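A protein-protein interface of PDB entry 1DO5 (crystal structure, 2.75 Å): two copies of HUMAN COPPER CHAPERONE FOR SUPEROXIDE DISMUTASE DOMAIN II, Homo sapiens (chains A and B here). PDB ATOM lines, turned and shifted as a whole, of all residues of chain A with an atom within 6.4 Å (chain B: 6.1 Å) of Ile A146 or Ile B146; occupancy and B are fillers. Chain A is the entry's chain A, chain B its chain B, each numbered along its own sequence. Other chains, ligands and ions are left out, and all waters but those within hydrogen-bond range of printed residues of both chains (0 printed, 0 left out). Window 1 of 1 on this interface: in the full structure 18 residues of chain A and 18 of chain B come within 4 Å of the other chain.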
ATOM      1  N   VAL A   7     -20.395 -36.078 -18.017  1.00  0.00           N
ATOM      2  CA  VAL A   7     -21.110 -35.366 -19.058  1.00  0.00           C
ATOM      3  C   VAL A   7     -20.344 -34.097 -19.379  1.00  0.00           C
ATOM      4  O   VAL A   7     -19.734 -33.496 -18.502  1.00  0.00           O
ATOM      5  CB  VAL A   7     -22.554 -35.009 -18.632  1.00  0.00           C
ATOM      6  CG1 VAL A   7     -22.553 -34.154 -17.392  1.00  0.00           C
ATOM      7  CG2 VAL A   7     -23.246 -34.285 -19.757  1.00  0.00           C
ATOM      8  N   ALA A   8     -20.347 -33.706 -20.643  1.00  0.00           N
ATOM      9  CA  ALA A   8     -19.651 -32.492 -21.035  1.00  0.00           C
ATOM     10  C   ALA A   8     -20.570 -31.648 -21.895  1.00  0.00           C
ATOM     11  O   ALA A   8     -20.845 -31.986 -23.040  1.00  0.00           O
ATOM     12  CB  ALA A   8     -18.368 -32.828 -21.794  1.00  0.00           C
ATOM     13  N   ILE A   9     -21.058 -30.558 -21.321  1.00  0.00           N
ATOM     14  CA  ILE A   9     -21.936 -29.641 -22.028  1.00  0.00           C
ATOM     15  C   ILE A   9     -21.052 -28.717 -22.858  1.00  0.00           C
ATOM     16  O   ILE A   9     -20.180 -28.049 -22.315  1.00  0.00           O
ATOM     17  CB  ILE A   9     -22.745 -28.788 -21.032  1.00  0.00           C
ATOM     18  CG1 ILE A   9     -23.531 -29.700 -20.085  1.00  0.00           C
ATOM     19  CG2 ILE A   9     -23.661 -27.855 -21.789  1.00  0.00           C
ATOM     20  CD1 ILE A   9     -24.354 -28.969 -19.068  1.00  0.00           C
ATOM     21  N   LEU A  10     -21.265 -28.666 -24.168  1.00  0.00           N
ATOM     22  CA  LEU A  10     -20.433 -27.809 -25.005  1.00  0.00           C
ATOM     23  C   LEU A  10     -20.977 -26.412 -25.255  1.00  0.00           C
ATOM     24  O   LEU A  10     -22.128 -26.242 -25.630  1.00  0.00           O
ATOM     25  CB  LEU A  10     -20.151 -28.488 -26.340  1.00  0.00           C
ATOM     26  CG  LEU A  10     -19.216 -29.693 -26.279  1.00  0.00           C
ATOM     27  CD1 LEU A  10     -18.779 -30.063 -27.682  1.00  0.00           C
ATOM     28  CD2 LEU A  10     -18.006 -29.359 -25.445  1.00  0.00           C
ATOM     29  N   GLY A  52      -9.796 -27.865 -17.574  1.00  0.00           N
ATOM     30  CA  GLY A  52     -11.203 -27.611 -17.786  1.00  0.00           C
ATOM     31  C   GLY A  52     -11.464 -26.160 -17.486  1.00  0.00           C
ATOM     32  O   GLY A  52     -12.609 -25.693 -17.511  1.00  0.00           O
ATOM     33  N   ASP A  53     -10.381 -25.447 -17.190  1.00  0.00           N
ATOM     34  CA  ASP A  53     -10.460 -24.031 -16.879  1.00  0.00           C
ATOM     35  C   ASP A  53     -11.002 -23.302 -18.089  1.00  0.00           C
ATOM     36  O   ASP A  53     -10.329 -23.228 -19.113  1.00  0.00           O
ATOM     37  CB  ASP A  53      -9.075 -23.475 -16.549  1.00  0.00           C
ATOM     38  CG  ASP A  53      -9.127 -22.045 -16.048  1.00  0.00           C
ATOM     39  OD1 ASP A  53      -9.928 -21.265 -16.601  1.00  0.00           O
ATOM     40  OD2 ASP A  53      -8.366 -21.699 -15.113  1.00  0.00           O
ATOM     41  N   LEU A  54     -12.220 -22.784 -17.991  1.00  0.00           N
ATOM     42  CA  LEU A  54     -12.796 -22.049 -19.111  1.00  0.00           C
ATOM     43  C   LEU A  54     -12.767 -20.559 -18.796  1.00  0.00           C
ATOM     44  O   LEU A  54     -13.414 -19.743 -19.466  1.00  0.00           O
ATOM     45  CB  LEU A  54     -14.232 -22.494 -19.377  1.00  0.00           C
ATOM     46  CG  LEU A  54     -14.437 -23.935 -19.832  1.00  0.00           C
ATOM     47  CD1 LEU A  54     -15.902 -24.107 -20.216  1.00  0.00           C
ATOM     48  CD2 LEU A  54     -13.531 -24.266 -21.004  1.00  0.00           C
ATOM     49  N   VAL A 110     -10.147 -38.047 -17.753  1.00  0.00           N
ATOM     50  CA  VAL A 110     -10.695 -36.803 -18.272  1.00  0.00           C
ATOM     51  C   VAL A 110     -11.582 -35.946 -17.382  1.00  0.00           C
ATOM     52  O   VAL A 110     -11.911 -34.819 -17.755  1.00  0.00           O
ATOM     53  CB  VAL A 110     -11.450 -37.069 -19.585  1.00  0.00           C
ATOM     54  CG1 VAL A 110     -10.563 -37.832 -20.529  1.00  0.00           C
ATOM     55  CG2 VAL A 110     -12.718 -37.837 -19.315  1.00  0.00           C
ATOM     56  N   GLY A 112     -12.831 -33.263 -15.047  1.00  0.00           N
ATOM     57  CA  GLY A 112     -12.282 -31.992 -14.626  1.00  0.00           C
ATOM     58  C   GLY A 112     -11.616 -31.291 -15.781  1.00  0.00           C
ATOM     59  O   GLY A 112     -11.440 -30.077 -15.754  1.00  0.00           O
ATOM     60  N   ARG A 113     -11.237 -32.069 -16.790  1.00  0.00           N
ATOM     61  CA  ARG A 113     -10.590 -31.555 -17.992  1.00  0.00           C
ATOM     62  C   ARG A 113     -11.676 -31.047 -18.937  1.00  0.00           C
ATOM     63  O   ARG A 113     -12.786 -30.742 -18.498  1.00  0.00           O
ATOM     64  CB  ARG A 113      -9.809 -32.672 -18.663  1.00  0.00           C
ATOM     65  CG  ARG A 113      -8.877 -33.385 -17.714  1.00  0.00           C
ATOM     66  CD  ARG A 113      -8.034 -34.415 -18.428  1.00  0.00           C
ATOM     67  NE  ARG A 113      -7.090 -35.033 -17.513  1.00  0.00           N
ATOM     68  CZ  ARG A 113      -6.120 -34.370 -16.896  1.00  0.00           C
ATOM     69  NH1 ARG A 113      -5.969 -33.072 -17.106  1.00  0.00           N
ATOM     70  NH2 ARG A 113      -5.311 -34.999 -16.059  1.00  0.00           N
ATOM     71  N   SER A 114     -11.396 -30.964 -20.230  1.00  0.00           N
ATOM     72  CA  SER A 114     -12.442 -30.471 -21.102  1.00  0.00           C
ATOM     73  C   SER A 114     -12.512 -31.123 -22.463  1.00  0.00           C
ATOM     74  O   SER A 114     -11.517 -31.621 -22.989  1.00  0.00           O
ATOM     75  CB  SER A 114     -12.330 -28.949 -21.257  1.00  0.00           C
ATOM     76  OG  SER A 114     -11.068 -28.564 -21.778  1.00  0.00           O
ATOM     77  N   LEU A 115     -13.725 -31.124 -23.012  1.00  0.00           N
ATOM     78  CA  LEU A 115     -13.999 -31.679 -24.330  1.00  0.00           C
ATOM     79  C   LEU A 115     -14.145 -30.500 -25.278  1.00  0.00           C
ATOM     80  O   LEU A 115     -14.959 -29.611 -25.042  1.00  0.00           O
ATOM     81  CB  LEU A 115     -15.296 -32.493 -24.311  1.00  0.00           C
ATOM     82  CG  LEU A 115     -15.625 -33.157 -25.647  1.00  0.00           C
ATOM     83  CD1 LEU A 115     -14.421 -33.974 -26.111  1.00  0.00           C
ATOM     84  CD2 LEU A 115     -16.837 -34.040 -25.503  1.00  0.00           C
ATOM     85  N   CYS A 144     -16.318 -25.716 -26.212  1.00  0.00           N
ATOM     86  CA  CYS A 144     -15.718 -26.637 -25.257  1.00  0.00           C
ATOM     87  C   CYS A 144     -16.565 -26.808 -24.001  1.00  0.00           C
ATOM     88  O   CYS A 144     -17.246 -25.889 -23.560  1.00  0.00           O
ATOM     89  CB  CYS A 144     -14.329 -26.154 -24.866  1.00  0.00           C
ATOM     90  SG  CYS A 144     -14.340 -24.492 -24.140  1.00  0.00           S
ATOM     91  N   GLY A 145     -16.509 -27.998 -23.425  1.00  0.00           N
ATOM     92  CA  GLY A 145     -17.266 -28.259 -22.225  1.00  0.00           C
ATOM     93  C   GLY A 145     -16.395 -28.902 -21.171  1.00  0.00           C
ATOM     94  O   GLY A 145     -15.434 -29.615 -21.478  1.00  0.00           O
ATOM     95  N   ILE A 146     -16.727 -28.652 -19.914  1.00  0.00           N
ATOM     96  CA  ILE A 146     -15.975 -29.223 -18.823  1.00  0.00           C
ATOM     97  C   ILE A 146     -16.512 -30.614 -18.544  1.00  0.00           C
ATOM     98  O   ILE A 146     -17.682 -30.766 -18.231  1.00  0.00           O
ATOM     99  CB  ILE A 146     -16.118 -28.366 -17.576  1.00  0.00           C
ATOM    100  CG1 ILE A 146     -15.833 -26.912 -17.944  1.00  0.00           C
ATOM    101  CG2 ILE A 146     -15.164 -28.852 -16.495  1.00  0.00           C
ATOM    102  CD1 ILE A 146     -16.044 -25.946 -16.831  1.00  0.00           C
ATOM    103  N   ILE A 147     -15.672 -31.632 -18.683  1.00  0.00           N
ATOM    104  CA  ILE A 147     -16.101 -32.996 -18.418  1.00  0.00           C
ATOM    105  C   ILE A 147     -16.410 -33.090 -16.929  1.00  0.00           C
ATOM    106  O   ILE A 147     -15.531 -32.911 -16.092  1.00  0.00           O
ATOM    107  CB  ILE A 147     -14.993 -34.008 -18.789  1.00  0.00           C
ATOM    108  CG1 ILE A 147     -14.626 -33.864 -20.270  1.00  0.00           C
ATOM    109  CG2 ILE A 147     -15.470 -35.430 -18.506  1.00  0.00           C
ATOM    110  CD1 ILE A 147     -13.411 -34.684 -20.698  1.00  0.00           C
ATOM    111  N   ALA A 148     -17.664 -33.361 -16.596  1.00  0.00           N
ATOM    112  CA  ALA A 148     -18.076 -33.446 -15.197  1.00  0.00           C
ATOM    113  C   ALA A 148     -18.549 -34.833 -14.755  1.00  0.00           C
ATOM    114  O   ALA A 148     -19.040 -35.613 -15.564  1.00  0.00           O
ATOM    115  CB  ALA A 148     -19.177 -32.413 -14.932  1.00  0.00           C
ATOM    116  N   ARG A 149     -18.387 -35.137 -13.468  1.00  0.00           N
ATOM    117  CA  ARG A 149     -18.850 -36.416 -12.922  1.00  0.00           C
ATOM    118  C   ARG A 149     -20.357 -36.420 -13.074  1.00  0.00           C
ATOM    119  O   ARG A 149     -21.016 -35.407 -12.806  1.00  0.00           O
ATOM    120  CB  ARG A 149     -18.555 -36.543 -11.431  1.00  0.00           C
ATOM    121  CG  ARG A 149     -17.115 -36.474 -11.023  1.00  0.00           C
ATOM    122  CD  ARG A 149     -17.056 -36.414  -9.507  1.00  0.00           C
ATOM    123  NE  ARG A 149     -15.700 -36.279  -8.993  1.00  0.00           N
ATOM    124  CZ  ARG A 149     -14.775 -37.225  -9.094  1.00  0.00           C
ATOM    125  NH1 ARG A 149     -15.068 -38.376  -9.693  1.00  0.00           N
ATOM    126  NH2 ARG A 149     -13.560 -37.016  -8.600  1.00  0.00           N
ATOM    127  N   VAL B   7     -10.576 -24.722 -10.628  1.00  0.00           N
ATOM    128  CA  VAL B   7     -11.348 -23.497 -10.751  1.00  0.00           C
ATOM    129  C   VAL B   7     -12.814 -23.877 -10.939  1.00  0.00           C
ATOM    130  O   VAL B   7     -13.119 -24.973 -11.405  1.00  0.00           O
ATOM    131  CB  VAL B   7     -10.891 -22.664 -11.966  1.00  0.00           C
ATOM    132  CG1 VAL B   7     -11.626 -21.332 -11.989  1.00  0.00           C
ATOM    133  CG2 VAL B   7      -9.396 -22.435 -11.909  1.00  0.00           C
ATOM    134  N   ALA B   8     -13.712 -22.980 -10.565  1.00  0.00           N
ATOM    135  CA  ALA B   8     -15.129 -23.229 -10.720  1.00  0.00           C
ATOM    136  C   ALA B   8     -15.781 -21.918 -11.089  1.00  0.00           C
ATOM    137  O   ALA B   8     -15.737 -20.956 -10.326  1.00  0.00           O
ATOM    138  CB  ALA B   8     -15.727 -23.765  -9.430  1.00  0.00           C
ATOM    139  N   ILE B   9     -16.375 -21.875 -12.272  1.00  0.00           N
ATOM    140  CA  ILE B   9     -17.049 -20.678 -12.735  1.00  0.00           C
ATOM    141  C   ILE B   9     -18.510 -20.781 -12.345  1.00  0.00           C
ATOM    142  O   ILE B   9     -19.254 -21.534 -12.955  1.00  0.00           O
ATOM    143  CB  ILE B   9     -16.939 -20.546 -14.259  1.00  0.00           C
ATOM    144  CG1 ILE B   9     -15.484 -20.288 -14.650  1.00  0.00           C
ATOM    145  CG2 ILE B   9     -17.820 -19.421 -14.742  1.00  0.00           C
ATOM    146  CD1 ILE B   9     -15.246 -20.231 -16.137  1.00  0.00           C
ATOM    147  N   LEU B  10     -18.912 -20.032 -11.321  1.00  0.00           N
ATOM    148  CA  LEU B  10     -20.293 -20.046 -10.849  1.00  0.00           C
ATOM    149  C   LEU B  10     -21.208 -19.187 -11.705  1.00  0.00           C
ATOM    150  O   LEU B  10     -20.754 -18.315 -12.446  1.00  0.00           O
ATOM    151  CB  LEU B  10     -20.382 -19.565  -9.400  1.00  0.00           C
ATOM    152  CG  LEU B  10     -19.856 -20.489  -8.302  1.00  0.00           C
ATOM    153  CD1 LEU B  10     -20.051 -19.851  -6.934  1.00  0.00           C
ATOM    154  CD2 LEU B  10     -20.597 -21.793  -8.367  1.00  0.00           C
ATOM    155  N   GLY B  52     -20.889 -32.571 -11.310  1.00  0.00           N
ATOM    156  CA  GLY B  52     -20.743 -31.275 -11.945  1.00  0.00           C
ATOM    157  C   GLY B  52     -21.676 -31.195 -13.143  1.00  0.00           C
ATOM    158  O   GLY B  52     -21.609 -30.268 -13.957  1.00  0.00           O
ATOM    159  N   ASP B  53     -22.553 -32.189 -13.246  1.00  0.00           N
ATOM    160  CA  ASP B  53     -23.526 -32.276 -14.321  1.00  0.00           C
ATOM    161  C   ASP B  53     -24.577 -31.171 -14.246  1.00  0.00           C
ATOM    162  O   ASP B  53     -25.529 -31.269 -13.486  1.00  0.00           O
ATOM    163  CB  ASP B  53     -24.215 -33.629 -14.257  1.00  0.00           C
ATOM    164  CG  ASP B  53     -25.341 -33.759 -15.256  1.00  0.00           C
ATOM    165  OD1 ASP B  53     -25.828 -32.726 -15.749  1.00  0.00           O
ATOM    166  OD2 ASP B  53     -25.751 -34.904 -15.537  1.00  0.00           O
ATOM    167  N   LEU B  54     -24.423 -30.138 -15.064  1.00  0.00           N
ATOM    168  CA  LEU B  54     -25.364 -29.026 -15.071  1.00  0.00           C
ATOM    169  C   LEU B  54     -26.467 -29.182 -16.121  1.00  0.00           C
ATOM    170  O   LEU B  54     -27.201 -28.241 -16.412  1.00  0.00           O
ATOM    171  CB  LEU B  54     -24.609 -27.724 -15.315  1.00  0.00           C
ATOM    172  CG  LEU B  54     -23.448 -27.420 -14.378  1.00  0.00           C
ATOM    173  CD1 LEU B  54     -22.694 -26.192 -14.860  1.00  0.00           C
ATOM    174  CD2 LEU B  54     -23.983 -27.216 -12.981  1.00  0.00           C
ATOM    175  N   GLY B 112     -14.427 -32.266 -11.295  1.00  0.00           N
ATOM    176  CA  GLY B 112     -15.507 -32.912 -12.007  1.00  0.00           C
ATOM    177  C   GLY B 112     -16.807 -32.729 -11.257  1.00  0.00           C
ATOM    178  O   GLY B 112     -17.875 -33.022 -11.771  1.00  0.00           O
ATOM    179  N   ARG B 113     -16.714 -32.248 -10.026  1.00  0.00           N
ATOM    180  CA  ARG B 113     -17.898 -32.012  -9.205  1.00  0.00           C
ATOM    181  C   ARG B 113     -18.339 -30.551  -9.355  1.00  0.00           C
ATOM    182  O   ARG B 113     -18.057 -29.913 -10.372  1.00  0.00           O
ATOM    183  CB  ARG B 113     -17.592 -32.339  -7.739  1.00  0.00           C
ATOM    184  CG  ARG B 113     -17.085 -33.756  -7.520  1.00  0.00           C
ATOM    185  CD  ARG B 113     -16.934 -34.072  -6.046  1.00  0.00           C
ATOM    186  NE  ARG B 113     -16.300 -35.366  -5.836  1.00  0.00           N
ATOM    187  CZ  ARG B 113     -16.875 -36.536  -6.078  1.00  0.00           C
ATOM    188  NH1 ARG B 113     -18.116 -36.595  -6.536  1.00  0.00           N
ATOM    189  NH2 ARG B 113     -16.199 -37.650  -5.874  1.00  0.00           N
ATOM    190  N   SER B 114     -19.018 -30.015  -8.350  1.00  0.00           N
ATOM    191  CA  SER B 114     -19.472 -28.637  -8.450  1.00  0.00           C
ATOM    192  C   SER B 114     -19.498 -27.852  -7.144  1.00  0.00           C
ATOM    193  O   SER B 114     -19.633 -28.411  -6.051  1.00  0.00           O
ATOM    194  CB  SER B 114     -20.872 -28.595  -9.064  1.00  0.00           C
ATOM    195  OG  SER B 114     -21.825 -29.099  -8.151  1.00  0.00           O
ATOM    196  N   LEU B 115     -19.360 -26.538  -7.283  1.00  0.00           N
ATOM    197  CA  LEU B 115     -19.415 -25.628  -6.151  1.00  0.00           C
ATOM    198  C   LEU B 115     -20.783 -24.948  -6.313  1.00  0.00           C
ATOM    199  O   LEU B 115     -21.175 -24.607  -7.435  1.00  0.00           O
ATOM    200  CB  LEU B 115     -18.277 -24.612  -6.241  1.00  0.00           C
ATOM    201  CG  LEU B 115     -17.936 -23.842  -4.970  1.00  0.00           C
ATOM    202  CD1 LEU B 115     -17.687 -24.804  -3.814  1.00  0.00           C
ATOM    203  CD2 LEU B 115     -16.711 -23.000  -5.233  1.00  0.00           C
ATOM    204  N   CYS B 144     -24.141 -22.431  -9.355  1.00  0.00           N
ATOM    205  CA  CYS B 144     -23.228 -23.561  -9.275  1.00  0.00           C
ATOM    206  C   CYS B 144     -22.265 -23.610 -10.455  1.00  0.00           C
ATOM    207  O   CYS B 144     -22.581 -23.168 -11.554  1.00  0.00           O
ATOM    208  CB  CYS B 144     -24.020 -24.857  -9.221  1.00  0.00           C
ATOM    209  SG  CYS B 144     -25.080 -25.053 -10.678  1.00  0.00           S
ATOM    210  N   GLY B 145     -21.084 -24.165 -10.218  1.00  0.00           N
ATOM    211  CA  GLY B 145     -20.097 -24.269 -11.271  1.00  0.00           C
ATOM    212  C   GLY B 145     -19.367 -25.586 -11.160  1.00  0.00           C
ATOM    213  O   GLY B 145     -19.190 -26.107 -10.060  1.00  0.00           O
ATOM    214  N   ILE B 146     -18.957 -26.124 -12.304  1.00  0.00           N
ATOM    215  CA  ILE B 146     -18.237 -27.382 -12.348  1.00  0.00           C
ATOM    216  C   ILE B 146     -16.783 -27.148 -11.960  1.00  0.00           C
ATOM    217  O   ILE B 146     -16.084 -26.356 -12.609  1.00  0.00           O
ATOM    218  CB  ILE B 146     -18.257 -27.960 -13.748  1.00  0.00           C
ATOM    219  CG1 ILE B 146     -19.681 -27.936 -14.277  1.00  0.00           C
ATOM    220  CG2 ILE B 146     -17.699 -29.381 -13.741  1.00  0.00           C
ATOM    221  CD1 ILE B 146     -19.765 -28.300 -15.729  1.00  0.00           C
ATOM    222  N   ILE B 147     -16.342 -27.837 -10.907  1.00  0.00           N
ATOM    223  CA  ILE B 147     -14.978 -27.719 -10.410  1.00  0.00           C
ATOM    224  C   ILE B 147     -14.018 -28.342 -11.419  1.00  0.00           C
ATOM    225  O   ILE B 147     -13.915 -29.562 -11.503  1.00  0.00           O
ATOM    226  CB  ILE B 147     -14.841 -28.438  -9.053  1.00  0.00           C
ATOM    227  CG1 ILE B 147     -15.995 -28.024  -8.140  1.00  0.00           C
ATOM    228  CG2 ILE B 147     -13.513 -28.075  -8.393  1.00  0.00           C
ATOM    229  CD1 ILE B 147     -15.967 -28.675  -6.776  1.00  0.00           C
ATOM    230  N   ALA B 148     -13.305 -27.512 -12.174  1.00  0.00           N
ATOM    231  CA  ALA B 148     -12.390 -28.029 -13.199  1.00  0.00           C
ATOM    232  C   ALA B 148     -10.880 -27.987 -12.891  1.00  0.00           C
ATOM    233  O   ALA B 148     -10.423 -27.246 -12.017  1.00  0.00           O
ATOM    234  CB  ALA B 148     -12.667 -27.309 -14.523  1.00  0.00           C
ATOM    235  N   ARG B 149     -10.115 -28.796 -13.625  1.00  0.00           N
ATOM    236  CA  ARG B 149      -8.656 -28.854 -13.467  1.00  0.00           C
ATOM    237  C   ARG B 149      -8.028 -27.628 -14.121  1.00  0.00           C
ATOM    238  O   ARG B 149      -8.344 -27.297 -15.258  1.00  0.00           O
ATOM    239  CB  ARG B 149      -8.066 -30.095 -14.145  1.00  0.00           C
ATOM    240  CG  ARG B 149      -8.489 -31.456 -13.604  1.00  0.00           C
ATOM    241  CD  ARG B 149      -7.828 -32.516 -14.478  1.00  0.00           C
ATOM    242  NE  ARG B 149      -8.198 -33.899 -14.182  1.00  0.00           N
ATOM    243  CZ  ARG B 149      -7.814 -34.572 -13.104  1.00  0.00           C
ATOM    244  NH1 ARG B 149      -7.048 -34.000 -12.187  1.00  0.00           N
ATOM    245  NH2 ARG B 149      -8.177 -35.838 -12.955  1.00  0.00           N
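O of Val A7 lies within hydrogen-bond range of N of Ala A148 (2.8 Å). N of Gly A52 sits close to O of Gly A112 (3.3 Å). N of Gly A112 lies within hydrogen-bond range of O of Ile A147 (2.9 Å). O of Arg A113 sits at hydrogen-bond distance from N of Ile A147, 3.0 Å away. The backbone NH of Gly B112 lies within hydrogen-bond range of the backbone carbonyl oxygen of Ile B147 (2.8 Å). The backbone NH of Ile B147 sits at hydrogen-bond distance from the backbone carbonyl oxygen of Arg B113 (2.7 Å).
Of the 18 printed residues of chain A, 10 touch a printed residue of chain B. Hydrophobic or aromatic side chains of chain A that line the printed part of chain B: Val A7, Ile A9, Ile A146 and Ala A148. Among the printed residues, no Asp or Glu carboxylate lies within 4 Å of a Lys or Arg side-chain nitrogen of the other chain.
Val A7 touches Asp B53, and with the chains exchanged Asp A53 touches Val B7. Gly A52 touches Arg B149, and with the chains exchanged Arg A149 touches Gly B52. Asp A53 touches Arg B149, and with the chains exchanged Arg A149 touches Asp B53. Arg A113 touches Arg B149, and with the chains exchanged Arg A149 touches Arg B113. Positions printed for both chains: 7, 8, 9, 10, 52, 53, 54, 112, 113, 114, 115, 144, 145, 146, 147, 148 and 149. Of the 22 pairs that touch across the chains among the printed residues, 22 have their exchanged pair printed and touching as well.
Val A7 touches Asp B53. O of Gly A52 touches CB of Ala B148 (3.4 Å). Gly A112 touches Gly B112 (CA to N, 3.97 Å). O of Gly A112 touches CB of Ala B148 (3.3 Å). Arg A113 touches Arg B149 (NH1 to CD, 3.3 Å). Ile A146 touches Ile B146 (CG2 to CG2, 3.8 Å). Ala B148 touches Ile A146. Ala A148 touches Gly B52 (CB to C, 3.3 Å). CA of Ala A148 touches O of Gly B112, at 3.5 Å. Asp B53 touches Arg A149.
Ile A146 touches just these residues of chain B: Ile B146 and Ala B148. Of chain A, only Ile A146 and Ala A148 come within 4 Å of Ile B146. Of the printed residues of chain A, Val B7 touches Asp A53. Of the printed residues of chain A, Ile B9 touches Leu A54. Of the printed residues of chain A, Leu B54 touches Ile A9 (3.6 Å). Of the printed residues of chain B, Arg A149 touches Gly B52, Asp B53, Gly B112 and Arg B113. Printed residues of chain A within 4 Å of Arg B113: Arg A149. Gly B145 touches none of the printed residues of chain A. Cys A144 touches none of the printed residues of chain B. The nearest residue of chain B that does not touch Ile A146 is Ile B147 (5.2 Å). The nearest residue of chain A that does not touch Ile B146 is Ile A147 (4.8 Å). The nearest printed residue of chain A that does not touch Leu B54 is Val A7 (5.0 Å).
The backbone carbonyl oxygen (O) of Arg B149 is in hydrogen-bond range of the backbone NH (N) of Gly A52 (2.8 Å). N of Asp A53 is in hydrogen-bond range of O of Arg B149 (3.4 Å). The backbone carbonyl oxygen of Gly A112 lies within hydrogen-bond range of the backbone NH of Arg B149, at 2.8 Å. O of Arg A149 is in hydrogen-bond range of N of Gly B52, at 3.2 Å. The backbone NH (N) of Arg A149 is in hydrogen-bond range of the backbone carbonyl oxygen (O) of Gly B112, at 2.8 Å. The guanidinium group (NE) of Arg B113 lies close to the guanidinium group (NE) of Arg A149 (3.3 Å).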
